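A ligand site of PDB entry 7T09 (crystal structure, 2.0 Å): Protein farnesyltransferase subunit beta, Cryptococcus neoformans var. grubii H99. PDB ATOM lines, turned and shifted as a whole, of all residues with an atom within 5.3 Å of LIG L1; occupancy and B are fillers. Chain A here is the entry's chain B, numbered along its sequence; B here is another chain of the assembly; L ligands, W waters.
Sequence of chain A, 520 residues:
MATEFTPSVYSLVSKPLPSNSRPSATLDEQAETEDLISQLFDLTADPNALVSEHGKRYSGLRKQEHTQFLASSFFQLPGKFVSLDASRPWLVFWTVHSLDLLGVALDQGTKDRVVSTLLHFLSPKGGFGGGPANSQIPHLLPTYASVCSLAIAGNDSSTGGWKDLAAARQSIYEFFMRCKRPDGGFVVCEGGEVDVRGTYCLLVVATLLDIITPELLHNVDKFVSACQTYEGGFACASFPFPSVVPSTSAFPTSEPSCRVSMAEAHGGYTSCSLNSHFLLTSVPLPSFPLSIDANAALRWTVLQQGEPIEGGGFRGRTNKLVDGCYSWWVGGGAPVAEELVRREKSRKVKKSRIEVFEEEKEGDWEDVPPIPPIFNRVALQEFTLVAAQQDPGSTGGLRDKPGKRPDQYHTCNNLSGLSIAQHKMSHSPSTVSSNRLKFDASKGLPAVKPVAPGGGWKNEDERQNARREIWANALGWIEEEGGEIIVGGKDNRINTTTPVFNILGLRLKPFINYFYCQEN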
ATOM      1  N   TRP A  90      -1.670  27.763 -16.724  1.00  0.00           N
ATOM      2  CA  TRP A  90      -2.653  26.879 -16.110  1.00  0.00           C
ATOM      3  C   TRP A  90      -1.964  25.685 -15.470  1.00  0.00           C
ATOM      4  O   TRP A  90      -2.364  25.237 -14.381  1.00  0.00           O
ATOM      5  CB  TRP A  90      -3.684  26.402 -17.143  1.00  0.00           C
ATOM      6  CG  TRP A  90      -4.653  27.477 -17.555  1.00  0.00           C
ATOM      7  CD1 TRP A  90      -4.660  28.177 -18.726  1.00  0.00           C
ATOM      8  CD2 TRP A  90      -5.753  27.996 -16.773  1.00  0.00           C
ATOM      9  NE1 TRP A  90      -5.712  29.089 -18.730  1.00  0.00           N
ATOM     10  CE2 TRP A  90      -6.379  28.993 -17.542  1.00  0.00           C
ATOM     11  CE3 TRP A  90      -6.262  27.699 -15.493  1.00  0.00           C
ATOM     12  CZ2 TRP A  90      -7.498  29.709 -17.083  1.00  0.00           C
ATOM     13  CZ3 TRP A  90      -7.369  28.399 -15.047  1.00  0.00           C
ATOM     14  CH2 TRP A  90      -7.968  29.398 -15.832  1.00  0.00           C
ATOM     15  N   LEU A 141      -7.167  34.349 -20.353  1.00  0.00           N
ATOM     16  CA  LEU A 141      -7.246  33.195 -19.466  1.00  0.00           C
ATOM     17  C   LEU A 141      -5.884  32.920 -18.802  1.00  0.00           C
ATOM     18  O   LEU A 141      -5.848  32.723 -17.576  1.00  0.00           O
ATOM     19  CB  LEU A 141      -7.767  31.954 -20.203  1.00  0.00           C
ATOM     20  CG  LEU A 141      -9.282  31.740 -20.208  1.00  0.00           C
ATOM     21  CD1 LEU A 141     -10.037  32.972 -20.709  1.00  0.00           C
ATOM     22  CD2 LEU A 141      -9.628  30.515 -21.058  1.00  0.00           C
ATOM     23  N   ARG A 197     -16.014  32.928 -20.130  1.00  0.00           N
ATOM     24  CA  ARG A 197     -14.686  32.640 -19.572  1.00  0.00           C
ATOM     25  C   ARG A 197     -13.821  33.890 -19.588  1.00  0.00           C
ATOM     26  O   ARG A 197     -13.096  34.174 -18.617  1.00  0.00           O
ATOM     27  CB  ARG A 197     -13.973  31.511 -20.337  1.00  0.00           C
ATOM     28  CG  ARG A 197     -14.683  30.158 -20.401  1.00  0.00           C
ATOM     29  CD  ARG A 197     -13.978  29.237 -21.408  1.00  0.00           C
ATOM     30  NE  ARG A 197     -13.819  29.924 -22.684  1.00  0.00           N
ATOM     31  CZ  ARG A 197     -12.793  29.771 -23.517  1.00  0.00           C
ATOM     32  NH1 ARG A 197     -11.808  28.921 -23.233  1.00  0.00           N
ATOM     33  NH2 ARG A 197     -12.748  30.482 -24.643  1.00  0.00           N
ATOM     34  N   TYR A 200     -15.147  36.416 -16.931  1.00  0.00           N
ATOM     35  CA  TYR A 200     -14.791  35.975 -15.580  1.00  0.00           C
ATOM     36  C   TYR A 200     -13.324  36.249 -15.281  1.00  0.00           C
ATOM     37  O   TYR A 200     -12.985  36.814 -14.248  1.00  0.00           O
ATOM     38  CB  TYR A 200     -15.106  34.491 -15.391  1.00  0.00           C
ATOM     39  CG  TYR A 200     -14.424  33.900 -14.142  1.00  0.00           C
ATOM     40  CD1 TYR A 200     -14.938  34.148 -12.869  1.00  0.00           C
ATOM     41  CD2 TYR A 200     -13.269  33.124 -14.253  1.00  0.00           C
ATOM     42  CE1 TYR A 200     -14.308  33.627 -11.723  1.00  0.00           C
ATOM     43  CE2 TYR A 200     -12.642  32.597 -13.119  1.00  0.00           C
ATOM     44  CZ  TYR A 200     -13.166  32.851 -11.863  1.00  0.00           C
ATOM     45  OH  TYR A 200     -12.534  32.344 -10.749  1.00  0.00           O
ATOM     46  N   CYS A 201     -12.427  35.803 -16.183  1.00  0.00           N
ATOM     47  CA  CYS A 201     -11.004  35.964 -15.921  1.00  0.00           C
ATOM     48  C   CYS A 201     -10.634  37.442 -15.803  1.00  0.00           C
ATOM     49  O   CYS A 201      -9.840  37.825 -14.926  1.00  0.00           O
ATOM     50  CB  CYS A 201     -10.191  35.281 -17.022  1.00  0.00           C
ATOM     51  SG  CYS A 201     -10.252  33.469 -16.965  1.00  0.00           S
ATOM     52  N   HIS A 266     -24.162  25.138 -19.209  1.00  0.00           N
ATOM     53  CA  HIS A 266     -23.033  24.265 -18.862  1.00  0.00           C
ATOM     54  C   HIS A 266     -22.416  24.682 -17.537  1.00  0.00           C
ATOM     55  O   HIS A 266     -22.367  25.862 -17.204  1.00  0.00           O
ATOM     56  CB  HIS A 266     -21.949  24.257 -19.949  1.00  0.00           C
ATOM     57  CG  HIS A 266     -21.045  23.071 -19.864  1.00  0.00           C
ATOM     58  ND1 HIS A 266     -20.008  22.978 -18.966  1.00  0.00           N
ATOM     59  CD2 HIS A 266     -21.052  21.899 -20.548  1.00  0.00           C
ATOM     60  CE1 HIS A 266     -19.398  21.818 -19.107  1.00  0.00           C
ATOM     61  NE2 HIS A 266     -20.012  21.140 -20.072  1.00  0.00           N
ATOM     62  N   GLY A 268     -19.332  24.830 -16.606  1.00  0.00           N
ATOM     63  CA  GLY A 268     -18.197  25.735 -16.734  1.00  0.00           C
ATOM     64  C   GLY A 268     -18.613  27.174 -16.992  1.00  0.00           C
ATOM     65  O   GLY A 268     -18.045  28.105 -16.413  1.00  0.00           O
ATOM     66  N   TYR A 269     -19.614  27.368 -17.854  1.00  0.00           N
ATOM     67  CA  TYR A 269     -20.100  28.718 -18.161  1.00  0.00           C
ATOM     68  C   TYR A 269     -21.034  29.232 -17.080  1.00  0.00           C
ATOM     69  O   TYR A 269     -21.136  30.448 -16.887  1.00  0.00           O
ATOM     70  CB  TYR A 269     -20.804  28.713 -19.526  1.00  0.00           C
ATOM     71  CG  TYR A 269     -19.856  28.343 -20.652  1.00  0.00           C
ATOM     72  CD1 TYR A 269     -18.617  28.971 -20.765  1.00  0.00           C
ATOM     73  CD2 TYR A 269     -20.177  27.339 -21.564  1.00  0.00           C
ATOM     74  CE1 TYR A 269     -17.743  28.636 -21.799  1.00  0.00           C
ATOM     75  CE2 TYR A 269     -19.302  26.995 -22.577  1.00  0.00           C
ATOM     76  CZ  TYR A 269     -18.093  27.640 -22.690  1.00  0.00           C
ATOM     77  OH  TYR A 269     -17.221  27.313 -23.695  1.00  0.00           O
ATOM     78  N   CYS A 272     -18.641  30.587 -14.482  1.00  0.00           N
ATOM     79  CA  CYS A 272     -18.099  31.879 -14.897  1.00  0.00           C
ATOM     80  C   CYS A 272     -19.146  32.991 -14.799  1.00  0.00           C
ATOM     81  O   CYS A 272     -18.835  34.122 -14.398  1.00  0.00           O
ATOM     82  CB  CYS A 272     -17.533  31.780 -16.309  1.00  0.00           C
ATOM     83  SG  CYS A 272     -16.012  30.832 -16.359  1.00  0.00           S
ATOM     84  N   GLY A 316     -21.857  18.052 -16.040  1.00  0.00           N
ATOM     85  CA  GLY A 316     -21.669  19.397 -16.564  1.00  0.00           C
ATOM     86  C   GLY A 316     -22.889  19.948 -17.293  1.00  0.00           C
ATOM     87  O   GLY A 316     -23.021  21.164 -17.459  1.00  0.00           O
ATOM     88  N   ARG A 317     -23.778  19.060 -17.748  1.00  0.00           N
ATOM     89  CA  ARG A 317     -25.008  19.487 -18.404  1.00  0.00           C
ATOM     90  C   ARG A 317     -25.986  18.317 -18.413  1.00  0.00           C
ATOM     91  O   ARG A 317     -25.608  17.150 -18.258  1.00  0.00           O
ATOM     92  CB  ARG A 317     -24.758  20.027 -19.834  1.00  0.00           C
ATOM     93  CG  ARG A 317     -23.730  19.273 -20.688  1.00  0.00           C
ATOM     94  CD  ARG A 317     -23.551  19.876 -22.115  1.00  0.00           C
ATOM     95  NE  ARG A 317     -22.340  19.369 -22.753  1.00  0.00           N
ATOM     96  CZ  ARG A 317     -22.165  19.197 -24.062  1.00  0.00           C
ATOM     97  NH1 ARG A 317     -23.133  19.510 -24.927  1.00  0.00           N
ATOM     98  NH2 ARG A 317     -21.015  18.715 -24.509  1.00  0.00           N
ATOM     99  N   LYS A 320     -25.762  14.399 -19.789  1.00  0.00           N
ATOM    100  CA  LYS A 320     -24.357  14.010 -19.969  1.00  0.00           C
ATOM    101  C   LYS A 320     -23.862  13.297 -18.697  1.00  0.00           C
ATOM    102  O   LYS A 320     -24.655  12.923 -17.831  1.00  0.00           O
ATOM    103  CB  LYS A 320     -23.521  15.227 -20.345  1.00  0.00           C
ATOM    104  CG  LYS A 320     -23.870  15.762 -21.754  1.00  0.00           C
ATOM    105  CD  LYS A 320     -23.079  14.994 -22.774  1.00  0.00           C
ATOM    106  CE  LYS A 320     -22.025  15.863 -23.375  1.00  0.00           C
ATOM    107  NZ  LYS A 320     -20.831  15.057 -23.800  1.00  0.00           N
ATOM    108  N   LEU A 321     -22.538  13.076 -18.589  1.00  0.00           N
ATOM    109  CA  LEU A 321     -21.996  12.206 -17.544  1.00  0.00           C
ATOM    110  C   LEU A 321     -21.400  12.984 -16.364  1.00  0.00           C
ATOM    111  O   LEU A 321     -20.886  14.090 -16.521  1.00  0.00           O
ATOM    112  CB  LEU A 321     -20.914  11.268 -18.116  1.00  0.00           C
ATOM    113  CG  LEU A 321     -21.274  10.472 -19.384  1.00  0.00           C
ATOM    114  CD1 LEU A 321     -20.044   9.776 -19.964  1.00  0.00           C
ATOM    115  CD2 LEU A 321     -22.419   9.493 -19.118  1.00  0.00           C
ATOM    116  N   ASP A 323     -18.574  13.886 -13.621  1.00  0.00           N
ATOM    117  CA  ASP A 323     -17.158  14.131 -13.874  1.00  0.00           C
ATOM    118  C   ASP A 323     -16.625  14.927 -12.686  1.00  0.00           C
ATOM    119  O   ASP A 323     -17.195  15.960 -12.319  1.00  0.00           O
ATOM    120  CB  ASP A 323     -16.991  14.903 -15.212  1.00  0.00           C
ATOM    121  CG  ASP A 323     -15.532  15.294 -15.526  1.00  0.00           C
ATOM    122  OD1 ASP A 323     -15.240  15.559 -16.721  1.00  0.00           O
ATOM    123  OD2 ASP A 323     -14.676  15.351 -14.614  1.00  0.00           O
ATOM    124  N   TYR A 326     -16.344  18.902 -12.303  1.00  0.00           N
ATOM    125  CA  TYR A 326     -17.525  19.717 -12.017  1.00  0.00           C
ATOM    126  C   TYR A 326     -17.838  19.821 -10.538  1.00  0.00           C
ATOM    127  O   TYR A 326     -18.752  20.559 -10.172  1.00  0.00           O
ATOM    128  CB  TYR A 326     -18.730  19.158 -12.790  1.00  0.00           C
ATOM    129  CG  TYR A 326     -18.466  19.179 -14.271  1.00  0.00           C
ATOM    130  CD1 TYR A 326     -18.037  20.349 -14.902  1.00  0.00           C
ATOM    131  CD2 TYR A 326     -18.580  18.027 -15.042  1.00  0.00           C
ATOM    132  CE1 TYR A 326     -17.755  20.368 -16.272  1.00  0.00           C
ATOM    133  CE2 TYR A 326     -18.296  18.038 -16.416  1.00  0.00           C
ATOM    134  CZ  TYR A 326     -17.881  19.207 -17.027  1.00  0.00           C
ATOM    135  OH  TYR A 326     -17.617  19.219 -18.388  1.00  0.00           O
ATOM    136  N   TRP A 329     -16.680  23.369 -10.686  1.00  0.00           N
ATOM    137  CA  TRP A 329     -17.412  24.280 -11.577  1.00  0.00           C
ATOM    138  C   TRP A 329     -18.885  24.375 -11.188  1.00  0.00           C
ATOM    139  O   TRP A 329     -19.464  25.468 -11.209  1.00  0.00           O
ATOM    140  CB  TRP A 329     -17.282  23.849 -13.044  1.00  0.00           C
ATOM    141  CG  TRP A 329     -15.859  23.807 -13.520  1.00  0.00           C
ATOM    142  CD1 TRP A 329     -15.194  22.705 -13.967  1.00  0.00           C
ATOM    143  CD2 TRP A 329     -14.933  24.893 -13.592  1.00  0.00           C
ATOM    144  NE1 TRP A 329     -13.901  23.035 -14.311  1.00  0.00           N
ATOM    145  CE2 TRP A 329     -13.717  24.375 -14.079  1.00  0.00           C
ATOM    146  CE3 TRP A 329     -15.010  26.265 -13.289  1.00  0.00           C
ATOM    147  CZ2 TRP A 329     -12.581  25.173 -14.292  1.00  0.00           C
ATOM    148  CZ3 TRP A 329     -13.863  27.057 -13.485  1.00  0.00           C
ATOM    149  CH2 TRP A 329     -12.678  26.508 -13.988  1.00  0.00           C
ATOM    150  N   TYR A 409      -5.343  19.141 -14.307  1.00  0.00           N
ATOM    151  CA  TYR A 409      -6.593  19.897 -14.315  1.00  0.00           C
ATOM    152  C   TYR A 409      -7.663  19.241 -13.450  1.00  0.00           C
ATOM    153  O   TYR A 409      -8.356  19.920 -12.690  1.00  0.00           O
ATOM    154  CB  TYR A 409      -7.085  20.082 -15.769  1.00  0.00           C
ATOM    155  CG  TYR A 409      -8.567  20.375 -15.903  1.00  0.00           C
ATOM    156  CD1 TYR A 409      -9.040  21.693 -15.888  1.00  0.00           C
ATOM    157  CD2 TYR A 409      -9.493  19.354 -16.051  1.00  0.00           C
ATOM    158  CE1 TYR A 409     -10.416  21.976 -16.005  1.00  0.00           C
ATOM    159  CE2 TYR A 409     -10.867  19.628 -16.197  1.00  0.00           C
ATOM    160  CZ  TYR A 409     -11.311  20.929 -16.157  1.00  0.00           C
ATOM    161  OH  TYR A 409     -12.666  21.177 -16.261  1.00  0.00           O
ATOM    162  N   TYR B 123     -10.960  25.200 -29.268  1.00  0.00           N
ATOM    163  CA  TYR B 123     -11.641  26.488 -29.418  1.00  0.00           C
ATOM    164  C   TYR B 123     -11.073  27.271 -30.593  1.00  0.00           C
ATOM    165  O   TYR B 123     -11.809  27.966 -31.300  1.00  0.00           O
ATOM    166  CB  TYR B 123     -11.468  27.340 -28.151  1.00  0.00           C
ATOM    167  CG  TYR B 123     -12.360  27.079 -26.955  1.00  0.00           C
ATOM    168  CD1 TYR B 123     -13.584  27.731 -26.796  1.00  0.00           C
ATOM    169  CD2 TYR B 123     -11.937  26.220 -25.932  1.00  0.00           C
ATOM    170  CE1 TYR B 123     -14.386  27.500 -25.657  1.00  0.00           C
ATOM    171  CE2 TYR B 123     -12.717  25.992 -24.793  1.00  0.00           C
ATOM    172  CZ  TYR B 123     -13.939  26.636 -24.662  1.00  0.00           C
ATOM    173  OH  TYR B 123     -14.700  26.406 -23.535  1.00  0.00           O
ATOM    174  N   LYS B 157     -23.259  15.882 -29.475  1.00  0.00           N
ATOM    175  CA  LYS B 157     -23.384  16.836 -28.382  1.00  0.00           C
ATOM    176  C   LYS B 157     -22.201  17.795 -28.289  1.00  0.00           C
ATOM    177  O   LYS B 157     -22.105  18.552 -27.312  1.00  0.00           O
ATOM    178  CB  LYS B 157     -23.551  16.088 -27.049  1.00  0.00           C
ATOM    179  CG  LYS B 157     -24.790  15.185 -26.992  1.00  0.00           C
ATOM    180  CD  LYS B 157     -25.008  14.547 -25.602  1.00  0.00           C
ATOM    181  CE  LYS B 157     -26.271  13.649 -25.615  1.00  0.00           C
ATOM    182  NZ  LYS B 157     -26.596  13.151 -24.235  1.00  0.00           N
ATOM    183  N   TYR B 159     -20.149  20.691 -27.934  1.00  0.00           N
ATOM    184  CA  TYR B 159     -20.644  21.989 -27.486  1.00  0.00           C
ATOM    185  C   TYR B 159     -20.231  23.102 -28.444  1.00  0.00           C
ATOM    186  O   TYR B 159     -21.032  23.995 -28.752  1.00  0.00           O
ATOM    187  CB  TYR B 159     -20.139  22.291 -26.071  1.00  0.00           C
ATOM    188  CG  TYR B 159     -20.865  23.451 -25.433  1.00  0.00           C
ATOM    189  CD1 TYR B 159     -21.900  23.237 -24.524  1.00  0.00           C
ATOM    190  CD2 TYR B 159     -20.544  24.778 -25.764  1.00  0.00           C
ATOM    191  CE1 TYR B 159     -22.589  24.287 -23.946  1.00  0.00           C
ATOM    192  CE2 TYR B 159     -21.234  25.837 -25.206  1.00  0.00           C
ATOM    193  CZ  TYR B 159     -22.262  25.586 -24.289  1.00  0.00           C
ATOM    194  OH  TYR B 159     -22.953  26.621 -23.703  1.00  0.00           O
ATOM    195  N   HIS B 160     -18.983  23.068 -28.909  1.00  0.00           N
ATOM    196  CA  HIS B 160     -18.518  24.071 -29.874  1.00  0.00           C
ATOM    197  C   HIS B 160     -19.380  24.057 -31.133  1.00  0.00           C
ATOM    198  O   HIS B 160     -19.636  25.115 -31.716  1.00  0.00           O
ATOM    199  CB  HIS B 160     -17.056  23.828 -30.259  1.00  0.00           C
ATOM    200  CG  HIS B 160     -16.129  23.684 -29.092  1.00  0.00           C
ATOM    201  ND1 HIS B 160     -15.891  24.718 -28.205  1.00  0.00           N
ATOM    202  CD2 HIS B 160     -15.371  22.645 -28.674  1.00  0.00           C
ATOM    203  CE1 HIS B 160     -15.024  24.307 -27.287  1.00  0.00           C
ATOM    204  NE2 HIS B 160     -14.697  23.054 -27.556  1.00  0.00           N
HETATM  205  C1  LIG L   1     -17.828  20.881 -22.909  1.00  0.00           C
HETATM  206  O1  LIG L   1     -16.804  19.919 -23.053  1.00  0.00           O
HETATM  207  C2  LIG L   1     -17.375  22.086 -22.046  1.00  0.00           C
HETATM  208  C3  LIG L   1     -17.050  23.297 -22.540  1.00  0.00           C
HETATM  209  C4  LIG L   1     -17.117  23.601 -24.040  1.00  0.00           C
HETATM  210  C5  LIG L   1     -16.609  24.445 -21.603  1.00  0.00           C
HETATM  211  C6  LIG L   1     -16.401  24.014 -20.134  1.00  0.00           C
HETATM  212  C7  LIG L   1     -15.702  25.147 -19.335  1.00  0.00           C
HETATM  213  C8  LIG L   1     -15.196  24.938 -18.118  1.00  0.00           C
HETATM  214  C9  LIG L   1     -15.309  23.552 -17.446  1.00  0.00           C
HETATM  215  C10 LIG L   1     -14.496  26.014 -17.289  1.00  0.00           C
HETATM  216  C11 LIG L   1     -14.196  27.344 -17.984  1.00  0.00           C
HETATM  217  C12 LIG L   1     -13.674  28.342 -16.927  1.00  0.00           C
HETATM  218  C13 LIG L   1     -12.573  29.079 -17.042  1.00  0.00           C
HETATM  219  C14 LIG L   1     -11.656  29.043 -18.280  1.00  0.00           C
HETATM  220  C15 LIG L   1     -12.212  30.029 -15.892  1.00  0.00           C
HETATM  221  P1  LIG L   1     -17.096  18.283 -23.112  1.00  0.00           P
HETATM  222  O2  LIG L   1     -15.790  17.642 -23.488  1.00  0.00           O
HETATM  223  O3  LIG L   1     -18.208  17.981 -24.098  1.00  0.00           O
HETATM  224  O4  LIG L   1     -17.521  17.737 -21.639  1.00  0.00           O
HETATM  225  P2  LIG L   1     -19.020  17.433 -21.064  1.00  0.00           P
HETATM  226  O5  LIG L   1     -19.463  16.133 -21.685  1.00  0.00           O
HETATM  227  O6  LIG L   1     -19.974  18.549 -21.361  1.00  0.00           O
HETATM  228  O7  LIG L   1     -18.844  17.288 -19.551  1.00  0.00           O
HETATM  229  C1  LG2 L   2     -10.403  20.424 -22.309  1.00  0.00           C
HETATM  230  C2  LG2 L   2     -12.347  18.369 -20.132  1.00  0.00           C
HETATM  231  C3  LG2 L   2     -13.249  21.839 -19.690  1.00  0.00           C
HETATM  232  C4  LG2 L   2     -12.780  23.149 -19.774  1.00  0.00           C
HETATM  233  C5  LG2 L   2     -12.778  23.819 -20.998  1.00  0.00           C
HETATM  234  C6  LG2 L   2     -13.732  21.880 -22.061  1.00  0.00           C
HETATM  235  C7  LG2 L   2      -9.017  24.310 -19.570  1.00  0.00           C
HETATM  236  C8  LG2 L   2      -5.126  18.246 -18.747  1.00  0.00           C
HETATM  237  C9  LG2 L   2      -6.117  18.346 -19.914  1.00  0.00           C
HETATM  238  C10 LG2 L   2      -7.493  18.840 -19.460  1.00  0.00           C
HETATM  239  C11 LG2 L   2      -8.474  19.088 -20.632  1.00  0.00           C
HETATM  240  C12 LG2 L   2      -9.823  19.818 -20.126  1.00  0.00           C
HETATM  241  C13 LG2 L   2      -9.485  21.201 -19.681  1.00  0.00           C
HETATM  242  C14 LG2 L   2      -9.635  21.801 -22.102  1.00  0.00           C
HETATM  243  C15 LG2 L   2     -11.394  18.670 -21.315  1.00  0.00           C
HETATM  244  C16 LG2 L   2     -12.046  17.530 -19.077  1.00  0.00           C
HETATM  245  C17 LG2 L   2     -14.042  18.354 -18.768  1.00  0.00           C
HETATM  246  C18 LG2 L   2     -14.297  19.767 -20.814  1.00  0.00           C
HETATM  247  C19 LG2 L   2     -13.735  21.210 -20.837  1.00  0.00           C
HETATM  248  C20 LG2 L   2     -13.250  23.190 -22.142  1.00  0.00           C
HETATM  249  C21 LG2 L   2     -12.250  25.257 -21.100  1.00  0.00           C
HETATM  250  C22 LG2 L   2      -8.482  23.394 -20.461  1.00  0.00           C
HETATM  251  C23 LG2 L   2      -8.372  25.505 -19.278  1.00  0.00           C
HETATM  252  C24 LG2 L   2      -7.171  25.772 -19.916  1.00  0.00           C
HETATM  253  C25 LG2 L   2      -6.624  24.866 -20.822  1.00  0.00           C
HETATM  254  C26 LG2 L   2      -7.283  23.671 -21.095  1.00  0.00           C
HETATM  255  C27 LG2 L   2      -9.717  25.983 -17.313  1.00  0.00           C
HETATM  256  F1  LG2 L   2      -9.113  24.933 -16.684  1.00  0.00           F
HETATM  257  F2  LG2 L   2     -10.944  25.592 -17.749  1.00  0.00           F
HETATM  258  F3  LG2 L   2      -9.893  26.998 -16.425  1.00  0.00           F
HETATM  259  N1  LG2 L   2      -9.191  22.146 -20.733  1.00  0.00           N
HETATM  260  N2  LG2 L   2     -10.819  19.831 -21.125  1.00  0.00           N
HETATM  261  N3  LG2 L   2     -13.091  17.531 -18.259  1.00  0.00           N
HETATM  262  N4  LG2 L   2     -13.565  18.856 -19.922  1.00  0.00           N
HETATM  263  N5  LG2 L   2     -11.856  26.316 -21.175  1.00  0.00           N
HETATM  264  O1  LG2 L   2      -9.419  22.538 -23.019  1.00  0.00           O
HETATM  265  O2  LG2 L   2      -8.925  26.447 -18.380  1.00  0.00           O
HETATM  266  O   HOH W   1     -19.764  16.459 -26.457  1.00  0.00           O
HETATM  267  O   HOH W   2     -16.637  15.601 -18.989  1.00  0.00           O
HETATM  268  O   HOH W   3     -20.105  13.836 -20.405  1.00  0.00           O
HETATM  269  O   HOH W   4     -15.569  15.232 -25.010  1.00  0.00           O
HETATM  270  O   HOH W   5     -14.963  15.967 -21.196  1.00  0.00           O
HETATM  271  O   HOH W   6     -13.606  19.094 -24.541  1.00  0.00           O
HETATM  272  O   HOH W   7     -17.365  14.513 -22.434  1.00  0.00           O
HETATM  273  O   HOH W   8     -21.117  16.372 -18.068  1.00  0.00           O
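NH1 of Arg 317 sits at hydrogen-bond distance from O of Lys 157 of chain B (2.8 Å). ND1 of His 266 lies within hydrogen-bond range of N of Gly 268 (3.1 Å). The indole nitrogen (NE1) of Trp 329 sits at hydrogen-bond distance from the side-chain hydroxyl (OH) of Tyr 409. O of Gly 268 lies within hydrogen-bond range of SG of Cys 272. The backbone carbonyl oxygen (O) of Arg 197 lies within hydrogen-bond range of the side-chain sulfur (SG) of Cys 201. The side-chain hydroxyl of Tyr 123 of chain B sits at hydrogen-bond distance from the side-chain hydroxyl of Tyr 269, 2.7 Å away.
O5 of LIG L1 lies within salt-bridge range of NZ of Lys 320, 2.7 Å away. A ring nitrogen (NE2) of His 266 is in hydrogen-bond range of an oxygen (O6) of LIG L1 (2.9 Å). The side-chain hydroxyl (OH) of Tyr 326 is in hydrogen-bond range of an oxygen (O7) of LIG L1 (2.6 Å). The guanidinium group of Arg 317 is in salt-bridge range of an oxygen (O6) of LIG L1 (2.9 Å). NH1 of Arg 197 sits at hydrogen-bond distance from N5 of LG2 L2 (3.3 Å).
Water W3 lies within hydrogen-bond range of an oxygen (O5) of LIG L1 (2.7 Å) and the backbone NH (N) of Leu 321 (3.1 Å). Water W8 lies within hydrogen-bond range of the backbone NH (N) of Gly 316, the backbone carbonyl oxygen (O) of Leu 321 and an oxygen (O7) of LIG L1. Water W1 lies within hydrogen-bond range of NZ of Lys 320 (3.2 Å), O3 of LIG L1 (3.2 Å), NH2 of Arg 317 (3.2 Å) and O of Lys 157 of chain B (3.3 Å).
CD2 of Leu 141 touches C14 of LIG L1, at 3.7 Å. Arg 197 touches LIG L1 (CG to C11, 3.7 Å). Tyr 200 touches LIG L1 (CD2 to C15, 3.7 Å). Gly 268 touches LIG L1 (CA to C8, 3.4 Å). Tyr 269 touches LIG L1 (OH to C5, 3.6 Å). Cys 272 touches LIG L1 (SG to C12, 3.5 Å). Trp 329 touches LIG L1. Tyr 409 touches LIG L1 (OH to C9, 3.7 Å). Tyr 123 of chain B touches LIG L1. Tyr 159 of chain B touches LIG L1 (CB to C4, 3.9 Å). His 160 of chain B touches LIG L1. Hydrophobic or aromatic side chains within 4 Å of LIG L1: Leu 141, Tyr 200, His 266, Tyr 269, Tyr 326, Trp 329, Tyr 159 of chain B and His 160 of chain B. The nearest printed residue that does not touch LIG L1 is Cys 201 (4.1 Å).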
